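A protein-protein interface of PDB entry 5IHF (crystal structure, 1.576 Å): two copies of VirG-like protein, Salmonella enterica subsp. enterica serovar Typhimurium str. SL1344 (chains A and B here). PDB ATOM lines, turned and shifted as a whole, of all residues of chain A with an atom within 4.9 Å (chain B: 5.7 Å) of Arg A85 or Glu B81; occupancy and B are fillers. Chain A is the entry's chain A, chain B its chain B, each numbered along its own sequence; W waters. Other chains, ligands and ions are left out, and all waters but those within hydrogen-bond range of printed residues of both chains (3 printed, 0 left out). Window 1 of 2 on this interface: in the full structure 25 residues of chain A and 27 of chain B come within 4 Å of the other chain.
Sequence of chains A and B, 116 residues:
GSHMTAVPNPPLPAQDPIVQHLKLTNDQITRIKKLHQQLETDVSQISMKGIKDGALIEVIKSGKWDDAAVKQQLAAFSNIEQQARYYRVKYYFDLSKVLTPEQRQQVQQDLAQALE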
ATOM      1  N   ALA A   6     -27.380   9.703  17.930  1.00  0.00           N
ATOM      2  CA  ALA A   6     -26.749   8.876  18.954  1.00  0.00           C
ATOM      3  C   ALA A   6     -25.589   9.624  19.604  1.00  0.00           C
ATOM      4  O   ALA A   6     -25.719  10.145  20.713  1.00  0.00           O
ATOM      5  CB  ALA A   6     -26.271   7.562  18.353  1.00  0.00           C
ATOM      6  N   VAL A   7     -24.459   9.669  18.904  1.00  0.00           N
ATOM      7  CA  VAL A   7     -23.295  10.422  19.351  1.00  0.00           C
ATOM      8  C   VAL A   7     -22.709  11.174  18.155  1.00  0.00           C
ATOM      9  O   VAL A   7     -22.411  10.558  17.130  1.00  0.00           O
ATOM     10  CB  VAL A   7     -22.218   9.508  19.970  1.00  0.00           C
ATOM     11  CG1 VAL A   7     -21.038  10.332  20.469  1.00  0.00           C
ATOM     12  CG2 VAL A   7     -22.807   8.684  21.105  1.00  0.00           C
ATOM     13  N   SER A  78     -23.523  -2.252  13.057  1.00  0.00           N
ATOM     14  CA  SER A  78     -23.797  -1.700  14.372  1.00  0.00           C
ATOM     15  C   SER A  78     -22.680  -2.037  15.355  1.00  0.00           C
ATOM     16  O   SER A  78     -22.409  -1.266  16.273  1.00  0.00           O
ATOM     17  CB  SER A  78     -25.139  -2.201  14.892  1.00  0.00           C
ATOM     18  OG  SER A  78     -26.200  -1.449  14.331  1.00  0.00           O
ATOM     19  N   GLU A  81     -20.168   0.643  14.721  1.00  0.00           N
ATOM     20  CA  GLU A  81     -20.661   1.924  15.209  1.00  0.00           C
ATOM     21  C   GLU A  81     -20.598   2.028  16.733  1.00  0.00           C
ATOM     22  O   GLU A  81     -20.266   3.089  17.266  1.00  0.00           O
ATOM     23  CB  GLU A  81     -22.093   2.156  14.728  1.00  0.00           C
ATOM     24  CG  GLU A  81     -22.192   2.483  13.251  1.00  0.00           C
ATOM     25  CD  GLU A  81     -23.620   2.724  12.814  1.00  0.00           C
ATOM     26  OE1 GLU A  81     -24.487   1.891  13.146  1.00  0.00           O
ATOM     27  OE2 GLU A  81     -23.875   3.750  12.149  1.00  0.00           O
ATOM     28  N   GLN A  82     -20.907   0.937  17.431  1.00  0.00           N
ATOM     29  CA  GLN A  82     -20.825   0.923  18.891  1.00  0.00           C
ATOM     30  C   GLN A  82     -19.420   1.268  19.350  1.00  0.00           C
ATOM     31  O   GLN A  82     -19.237   2.027  20.297  1.00  0.00           O
ATOM     32  CB  GLN A  82     -21.215  -0.441  19.459  1.00  0.00           C
ATOM     33  CG  GLN A  82     -22.695  -0.725  19.451  1.00  0.00           C
ATOM     34  CD  GLN A  82     -23.013  -2.104  19.987  1.00  0.00           C
ATOM     35  OE1 GLN A  82     -23.608  -2.930  19.294  1.00  0.00           O
ATOM     36  NE2 GLN A  82     -22.613  -2.363  21.225  1.00  0.00           N
ATOM     37  N   GLN A  83     -18.431   0.698  18.671  1.00  0.00           N
ATOM     38  CA  GLN A  83     -17.035   0.912  19.030  1.00  0.00           C
ATOM     39  C   GLN A  83     -16.600   2.335  18.689  1.00  0.00           C
ATOM     40  O   GLN A  83     -15.909   2.987  19.475  1.00  0.00           O
ATOM     41  CB  GLN A  83     -16.135  -0.100  18.318  1.00  0.00           C
ATOM     42  CG  GLN A  83     -16.464  -1.553  18.628  1.00  0.00           C
ATOM     43  CD  GLN A  83     -15.627  -2.526  17.814  1.00  0.00           C
ATOM     44  OE1 GLN A  83     -14.397  -2.468  17.828  1.00  0.00           O
ATOM     45  NE2 GLN A  83     -16.293  -3.420  17.093  1.00  0.00           N
ATOM     46  N   ALA A  84     -16.999   2.816  17.515  1.00  0.00           N
ATOM     47  CA  ALA A  84     -16.637   4.164  17.095  1.00  0.00           C
ATOM     48  C   ALA A  84     -17.255   5.201  18.029  1.00  0.00           C
ATOM     49  O   ALA A  84     -16.600   6.171  18.424  1.00  0.00           O
ATOM     50  CB  ALA A  84     -17.076   4.412  15.659  1.00  0.00           C
ATOM     51  N   ARG A  85     -18.509   4.985  18.403  1.00  0.00           N
ATOM     52  CA  ARG A  85     -19.206   5.932  19.260  1.00  0.00           C
ATOM     53  C   ARG A  85     -18.603   5.958  20.658  1.00  0.00           C
ATOM     54  O   ARG A  85     -18.587   7.004  21.303  1.00  0.00           O
ATOM     55  CB  ARG A  85     -20.692   5.596  19.321  1.00  0.00           C
ATOM     56  CG  ARG A  85     -21.399   5.890  18.013  1.00  0.00           C
ATOM     57  CD  ARG A  85     -22.828   5.417  18.039  1.00  0.00           C
ATOM     58  NE  ARG A  85     -23.452   5.534  16.728  1.00  0.00           N
ATOM     59  CZ  ARG A  85     -24.659   5.061  16.443  1.00  0.00           C
ATOM     60  NH1 ARG A  85     -25.361   4.438  17.380  1.00  0.00           N
ATOM     61  NH2 ARG A  85     -25.162   5.204  15.224  1.00  0.00           N
ATOM     62  N   TYR A  86     -18.109   4.812  21.121  1.00  0.00           N
ATOM     63  CA  TYR A  86     -17.401   4.744  22.397  1.00  0.00           C
ATOM     64  C   TYR A  86     -16.241   5.732  22.380  1.00  0.00           C
ATOM     65  O   TYR A  86     -16.067   6.504  23.320  1.00  0.00           O
ATOM     66  CB  TYR A  86     -16.888   3.327  22.667  1.00  0.00           C
ATOM     67  CG  TYR A  86     -16.265   3.127  24.034  1.00  0.00           C
ATOM     68  CD1 TYR A  86     -14.944   3.484  24.279  1.00  0.00           C
ATOM     69  CD2 TYR A  86     -16.991   2.560  25.072  1.00  0.00           C
ATOM     70  CE1 TYR A  86     -14.374   3.294  25.522  1.00  0.00           C
ATOM     71  CE2 TYR A  86     -16.427   2.365  26.318  1.00  0.00           C
ATOM     72  CZ  TYR A  86     -15.118   2.735  26.536  1.00  0.00           C
ATOM     73  OH  TYR A  86     -14.554   2.542  27.776  1.00  0.00           O
ATOM     74  N   TYR A  87     -15.456   5.715  21.305  1.00  0.00           N
ATOM     75  CA  TYR A  87     -14.309   6.622  21.210  1.00  0.00           C
ATOM     76  C   TYR A  87     -14.769   8.075  21.104  1.00  0.00           C
ATOM     77  O   TYR A  87     -14.086   8.984  21.579  1.00  0.00           O
ATOM     78  CB  TYR A  87     -13.426   6.277  20.012  1.00  0.00           C
ATOM     79  CG  TYR A  87     -12.763   4.922  20.070  1.00  0.00           C
ATOM     80  CD1 TYR A  87     -11.987   4.546  21.157  1.00  0.00           C
ATOM     81  CD2 TYR A  87     -12.902   4.023  19.024  1.00  0.00           C
ATOM     82  CE1 TYR A  87     -11.378   3.307  21.202  1.00  0.00           C
ATOM     83  CE2 TYR A  87     -12.300   2.787  19.059  1.00  0.00           C
ATOM     84  CZ  TYR A  87     -11.541   2.432  20.149  1.00  0.00           C
ATOM     85  OH  TYR A  87     -10.940   1.194  20.181  1.00  0.00           O
ATOM     86  N   ARG A  88     -15.914   8.302  20.468  1.00  0.00           N
ATOM     87  CA  ARG A  88     -16.427   9.660  20.314  1.00  0.00           C
ATOM     88  C   ARG A  88     -16.867  10.227  21.661  1.00  0.00           C
ATOM     89  O   ARG A  88     -16.614  11.393  21.961  1.00  0.00           O
ATOM     90  CB  ARG A  88     -17.586   9.692  19.317  1.00  0.00           C
ATOM     91  CG  ARG A  88     -17.164   9.388  17.895  1.00  0.00           C
ATOM     92  CD  ARG A  88     -18.364   9.216  16.990  1.00  0.00           C
ATOM     93  NE  ARG A  88     -17.980   8.697  15.682  1.00  0.00           N
ATOM     94  CZ  ARG A  88     -18.842   8.250  14.776  1.00  0.00           C
ATOM     95  NH1 ARG A  88     -20.143   8.257  15.033  1.00  0.00           N
ATOM     96  NH2 ARG A  88     -18.404   7.792  13.611  1.00  0.00           N
ATOM     97  N   VAL A  89     -17.529   9.406  22.471  1.00  0.00           N
ATOM     98  CA  VAL A  89     -17.910   9.822  23.812  1.00  0.00           C
ATOM     99  C   VAL A  89     -16.645  10.090  24.619  1.00  0.00           C
ATOM    100  O   VAL A  89     -16.552  11.094  25.329  1.00  0.00           O
ATOM    101  CB  VAL A  89     -18.778   8.759  24.514  1.00  0.00           C
ATOM    102  CG1 VAL A  89     -19.046   9.140  25.964  1.00  0.00           C
ATOM    103  CG2 VAL A  89     -20.095   8.588  23.776  1.00  0.00           C
ATOM    104  N   LYS A  90     -15.666   9.198  24.504  1.00  0.00           N
ATOM    105  CA  LYS A  90     -14.412   9.359  25.238  1.00  0.00           C
ATOM    106  C   LYS A  90     -13.707  10.651  24.836  1.00  0.00           C
ATOM    107  O   LYS A  90     -13.092  11.311  25.674  1.00  0.00           O
ATOM    108  CB  LYS A  90     -13.481   8.164  25.006  1.00  0.00           C
ATOM    109  CG  LYS A  90     -12.318   8.086  26.006  1.00  0.00           C
ATOM    110  CD  LYS A  90     -12.690   7.264  27.235  1.00  0.00           C
ATOM    111  CE  LYS A  90     -11.775   7.543  28.422  1.00  0.00           C
ATOM    112  NZ  LYS A  90     -10.328   7.448  28.079  1.00  0.00           N
ATOM    113  N   LEU B  74     -24.685   2.605  24.584  1.00  0.00           N
ATOM    114  CA  LEU B  74     -24.392   2.498  23.158  1.00  0.00           C
ATOM    115  C   LEU B  74     -24.913   1.185  22.582  1.00  0.00           C
ATOM    116  O   LEU B  74     -25.310   1.126  21.416  1.00  0.00           O
ATOM    117  CB  LEU B  74     -22.891   2.624  22.911  1.00  0.00           C
ATOM    118  CG  LEU B  74     -22.309   4.003  23.218  1.00  0.00           C
ATOM    119  CD1 LEU B  74     -20.807   3.996  23.011  1.00  0.00           C
ATOM    120  CD2 LEU B  74     -22.958   5.085  22.365  1.00  0.00           C
ATOM    121  N   ALA B  76     -27.593  -0.209  23.630  1.00  0.00           N
ATOM    122  CA  ALA B  76     -29.031   0.016  23.524  1.00  0.00           C
ATOM    123  C   ALA B  76     -29.374   0.762  22.236  1.00  0.00           C
ATOM    124  O   ALA B  76     -30.333   0.410  21.546  1.00  0.00           O
ATOM    125  CB  ALA B  76     -29.538   0.780  24.733  1.00  0.00           C
ATOM    126  N   PHE B  77     -28.594   1.794  21.919  1.00  0.00           N
ATOM    127  CA  PHE B  77     -28.737   2.508  20.652  1.00  0.00           C
ATOM    128  C   PHE B  77     -28.582   1.542  19.486  1.00  0.00           C
ATOM    129  O   PHE B  77     -29.380   1.550  18.546  1.00  0.00           O
ATOM    130  CB  PHE B  77     -27.691   3.622  20.512  1.00  0.00           C
ATOM    131  CG  PHE B  77     -27.898   4.800  21.425  1.00  0.00           C
ATOM    132  CD1 PHE B  77     -29.146   5.105  21.943  1.00  0.00           C
ATOM    133  CD2 PHE B  77     -26.828   5.617  21.752  1.00  0.00           C
ATOM    134  CE1 PHE B  77     -29.316   6.198  22.776  1.00  0.00           C
ATOM    135  CE2 PHE B  77     -26.992   6.707  22.582  1.00  0.00           C
ATOM    136  CZ  PHE B  77     -28.238   6.998  23.095  1.00  0.00           C
ATOM    137  N   SER B  78     -27.534   0.727  19.555  1.00  0.00           N
ATOM    138  CA  SER B  78     -27.227  -0.260  18.522  1.00  0.00           C
ATOM    139  C   SER B  78     -28.418  -1.158  18.235  1.00  0.00           C
ATOM    140  O   SER B  78     -28.811  -1.334  17.082  1.00  0.00           O
ATOM    141  CB  SER B  78     -26.041  -1.119  18.948  1.00  0.00           C
ATOM    142  OG  SER B  78     -25.889  -2.239  18.098  1.00  0.00           O
ATOM    143  N   ASN B  79     -28.981  -1.723  19.297  1.00  0.00           N
ATOM    144  CA  ASN B  79     -30.078  -2.673  19.178  1.00  0.00           C
ATOM    145  C   ASN B  79     -31.291  -2.050  18.496  1.00  0.00           C
ATOM    146  O   ASN B  79     -31.905  -2.665  17.632  1.00  0.00           O
ATOM    147  CB  ASN B  79     -30.461  -3.205  20.562  1.00  0.00           C
ATOM    148  CG  ASN B  79     -31.631  -4.168  20.517  1.00  0.00           C
ATOM    149  OD1 ASN B  79     -31.581  -5.190  19.834  1.00  0.00           O
ATOM    150  ND2 ASN B  79     -32.687  -3.853  21.261  1.00  0.00           N
ATOM    151  N   ILE B  80     -31.623  -0.822  18.877  1.00  0.00           N
ATOM    152  CA  ILE B  80     -32.751  -0.114  18.280  1.00  0.00           C
ATOM    153  C   ILE B  80     -32.500   0.176  16.801  1.00  0.00           C
ATOM    154  O   ILE B  80     -33.371  -0.047  15.957  1.00  0.00           O
ATOM    155  CB  ILE B  80     -33.030   1.207  19.029  1.00  0.00           C
ATOM    156  CG1 ILE B  80     -33.575   0.904  20.424  1.00  0.00           C
ATOM    157  CG2 ILE B  80     -34.030   2.079  18.266  1.00  0.00           C
ATOM    158  CD1 ILE B  80     -33.386   2.031  21.407  1.00  0.00           C
ATOM    159  N   GLU B  81     -31.307   0.670  16.488  1.00  0.00           N
ATOM    160  CA  GLU B  81     -30.963   1.044  15.121  1.00  0.00           C
ATOM    161  C   GLU B  81     -30.917  -0.159  14.186  1.00  0.00           C
ATOM    162  O   GLU B  81     -31.328  -0.059  13.031  1.00  0.00           O
ATOM    163  CB  GLU B  81     -29.623   1.774  15.096  1.00  0.00           C
ATOM    164  CG  GLU B  81     -29.701   3.190  15.615  1.00  0.00           C
ATOM    165  CD  GLU B  81     -28.343   3.853  15.673  1.00  0.00           C
ATOM    166  OE1 GLU B  81     -27.393   3.204  16.160  1.00  0.00           O
ATOM    167  OE2 GLU B  81     -28.223   5.012  15.226  1.00  0.00           O
ATOM    168  N   GLN B  82     -30.419  -1.291  14.680  1.00  0.00           N
ATOM    169  CA  GLN B  82     -30.382  -2.521  13.888  1.00  0.00           C
ATOM    170  C   GLN B  82     -31.783  -2.885  13.426  1.00  0.00           C
ATOM    171  O   GLN B  82     -31.990  -3.290  12.277  1.00  0.00           O
ATOM    172  CB  GLN B  82     -29.796  -3.680  14.696  1.00  0.00           C
ATOM    173  CG  GLN B  82     -28.290  -3.782  14.675  1.00  0.00           C
ATOM    174  CD  GLN B  82     -27.792  -4.982  15.455  1.00  0.00           C
ATOM    175  OE1 GLN B  82     -28.099  -6.126  15.119  1.00  0.00           O
ATOM    176  NE2 GLN B  82     -27.035  -4.725  16.513  1.00  0.00           N
ATOM    177  N   GLN B  83     -32.743  -2.733  14.333  1.00  0.00           N
ATOM    178  CA  GLN B  83     -34.135  -3.069  14.054  1.00  0.00           C
ATOM    179  C   GLN B  83     -34.758  -2.073  13.092  1.00  0.00           C
ATOM    180  O   GLN B  83     -35.431  -2.462  12.137  1.00  0.00           O
ATOM    181  CB  GLN B  83     -34.946  -3.114  15.348  1.00  0.00           C
ATOM    182  CG  GLN B  83     -34.491  -4.184  16.307  1.00  0.00           C
ATOM    183  CD  GLN B  83     -35.304  -4.196  17.581  1.00  0.00           C
ATOM    184  OE1 GLN B  83     -36.472  -4.581  17.583  1.00  0.00           O
ATOM    185  NE2 GLN B  83     -34.693  -3.755  18.673  1.00  0.00           N
ATOM    186  N   ALA B  84     -34.541  -0.786  13.342  1.00  0.00           N
ATOM    187  CA  ALA B  84     -35.099   0.243  12.474  1.00  0.00           C
ATOM    188  C   ALA B  84     -34.568   0.077  11.057  1.00  0.00           C
ATOM    189  O   ALA B  84     -35.327   0.147  10.090  1.00  0.00           O
ATOM    190  CB  ALA B  84     -34.779   1.628  13.004  1.00  0.00           C
ATOM    191  N   ARG B  85     -33.268  -0.165  10.934  1.00  0.00           N
ATOM    192  CA  ARG B  85     -32.648  -0.299   9.625  1.00  0.00           C
ATOM    193  C   ARG B  85     -33.134  -1.543   8.888  1.00  0.00           C
ATOM    194  O   ARG B  85     -33.214  -1.540   7.663  1.00  0.00           O
ATOM    195  CB  ARG B  85     -31.127  -0.330   9.759  1.00  0.00           C
ATOM    196  CG  ARG B  85     -30.540   0.997  10.196  1.00  0.00           C
ATOM    197  CD  ARG B  85     -29.069   0.874  10.490  1.00  0.00           C
ATOM    198  NE  ARG B  85     -28.528   2.116  11.033  1.00  0.00           N
ATOM    199  CZ  ARG B  85     -27.332   2.220  11.600  1.00  0.00           C
ATOM    200  NH1 ARG B  85     -26.551   1.154  11.700  1.00  0.00           N
ATOM    201  NH2 ARG B  85     -26.920   3.390  12.071  1.00  0.00           N
ATOM    202  N   TYR B  86     -33.452  -2.600   9.627  1.00  0.00           N
ATOM    203  CA  TYR B  86     -34.030  -3.799   9.022  1.00  0.00           C
ATOM    204  C   TYR B  86     -35.262  -3.425   8.209  1.00  0.00           C
ATOM    205  O   TYR B  86     -35.401  -3.825   7.052  1.00  0.00           O
ATOM    206  CB  TYR B  86     -34.396  -4.831  10.092  1.00  0.00           C
ATOM    207  CG  TYR B  86     -35.147  -6.034   9.563  1.00  0.00           C
ATOM    208  CD1 TYR B  86     -36.533  -6.038   9.501  1.00  0.00           C
ATOM    209  CD2 TYR B  86     -34.468  -7.168   9.136  1.00  0.00           C
ATOM    210  CE1 TYR B  86     -37.224  -7.136   9.022  1.00  0.00           C
ATOM    211  CE2 TYR B  86     -35.151  -8.271   8.655  1.00  0.00           C
ATOM    212  CZ  TYR B  86     -36.524  -8.247   8.603  1.00  0.00           C
ATOM    213  OH  TYR B  86     -37.199  -9.344   8.126  1.00  0.00           O
ATOM    214  N   ARG B  88     -36.122  -0.405   7.180  1.00  0.00           N
ATOM    215  CA  ARG B  88     -35.787   0.545   6.128  1.00  0.00           C
ATOM    216  C   ARG B  88     -35.300  -0.187   4.880  1.00  0.00           C
ATOM    217  O   ARG B  88     -35.699   0.148   3.763  1.00  0.00           O
ATOM    218  CB  ARG B  88     -34.743   1.543   6.625  1.00  0.00           C
ATOM    219  CG  ARG B  88     -35.299   2.441   7.715  1.00  0.00           C
ATOM    220  CD  ARG B  88     -34.237   3.291   8.388  1.00  0.00           C
ATOM    221  NE  ARG B  88     -34.812   4.038   9.504  1.00  0.00           N
ATOM    222  CZ  ARG B  88     -34.102   4.639  10.453  1.00  0.00           C
ATOM    223  NH1 ARG B  88     -32.780   4.585  10.436  1.00  0.00           N
ATOM    224  NH2 ARG B  88     -34.720   5.293  11.428  1.00  0.00           N
HETATM  225  O   HOH W   1     -27.252  -1.559  11.929  1.00  0.00           O
HETATM  226  O   HOH W   2     -24.205   2.581  19.345  1.00  0.00           O
HETATM  227  O   HOH W   3     -25.941   1.299  15.143  1.00  0.00           O
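NH1 of Arg B85 lies within salt-bridge range of OE1 of Glu A81 (2.6 Å).
OE1 of Glu B81 is in salt-bridge range of NH1 of Arg A85 (2.7 Å).
OG of Ser B78 is in hydrogen-bond range of OE1 of Gln A82 (2.7 Å).
NH2 of Arg A85 is in salt-bridge range of OE2 of Glu A81 (3.6 Å).
The guanidinium group (NH2) of Arg B85 is in salt-bridge range of the side-chain carboxylate (OE2) of Glu B81, 3.8 Å away.
The side-chain amide nitrogen (NE2) of Gln B82 lies within hydrogen-bond range of the side-chain hydroxyl (OG) of Ser B78, at 3.2 Å.
Water W3 lies within hydrogen-bond range of OE1 of Glu A81, OE1 of Glu B81, OG of Ser A78 and NH1 of Arg B85.
Water W1 bridges OG of Ser A78 (2.6 Å) and NH1 of Arg B85 (2.8 Å).
Water W2 lies within hydrogen-bond range of the backbone carbonyl oxygen (O) of Leu B74 and the guanidinium group (NH1) of Arg A85.
Of the 13 printed residues of chain B, 6 touch a printed residue of chain A.
Hydrophobic or aromatic side chains of chain B that line the printed part of chain A: Leu B74 and Phe B77.
Along chain B the printed residues that touch a printed residue of chain A span positions 74 to 85.
Of the 13 printed residues of chain A, 7 touch a printed residue of chain B.
Hydrophobic or aromatic side chains of chain A within 4 Å of the printed part of chain B: Ala A6, Val A7 and Tyr A86.
Among the printed residues, Asp or Glu carboxylates within 4 Å of a Lys or Arg side-chain nitrogen of the other chain: Glu A81 with Arg B85 (2.6 Å) and Arg A85 with Glu B81 (2.7 Å).
Of the printed residues of chain B, Val A7 touches Leu B74 (3.8 Å).
Printed residues of chain B within 4 Å of Ser A78: Ser B78, Gln B82 and Arg B85.
Gln A83 touches none of the printed residues of chain B.
Of the printed residues of chain B, Arg A85 touches Leu B74, Phe B77 and Glu B81.
Tyr A87 touches none of the printed residues of chain B.
Of chain A, only Arg A85 comes within 4 Å of Glu B81.
The nearest printed residue of chain B that does not touch Arg A85 is Arg B85 (4.04 Å).
The nearest residue of chain A that does not touch Glu B81 is Glu A81 (4.4 Å).
The nearest printed residue of chain A that does not touch Leu B74 is Val A89 (4.7 Å).
Ser B78 touches its own counterpart, Ser A78.
Ser A78 touches Gln B82, and with the chains exchanged Gln A82 touches Ser B78.
Ser A78 touches Arg B85, but with the chains exchanged Arg A85 does not touch Ser B78 (4.8 Å).
Glu A81 touches Arg B85, and with the chains exchanged Arg A85 touches Glu B81.
Among the printed residues, merely in contact across the chains: Ser A78 with Gln B82 (3.2 Å), Ser A78 with Ser B78 (3.3 Å), Tyr A86 with Leu B74 (3.4 Å), Gln A82 with Leu B74 (3.7 Å), Ser A78 with Arg B85 (3.7 Å), Arg A85 with Leu B74 (3.8 Å), Val A7 with Leu B74 (3.8 Å), Ala A6 with Phe B77 (3.96 Å) and Arg A85 with Phe B77 (3.99 Å).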
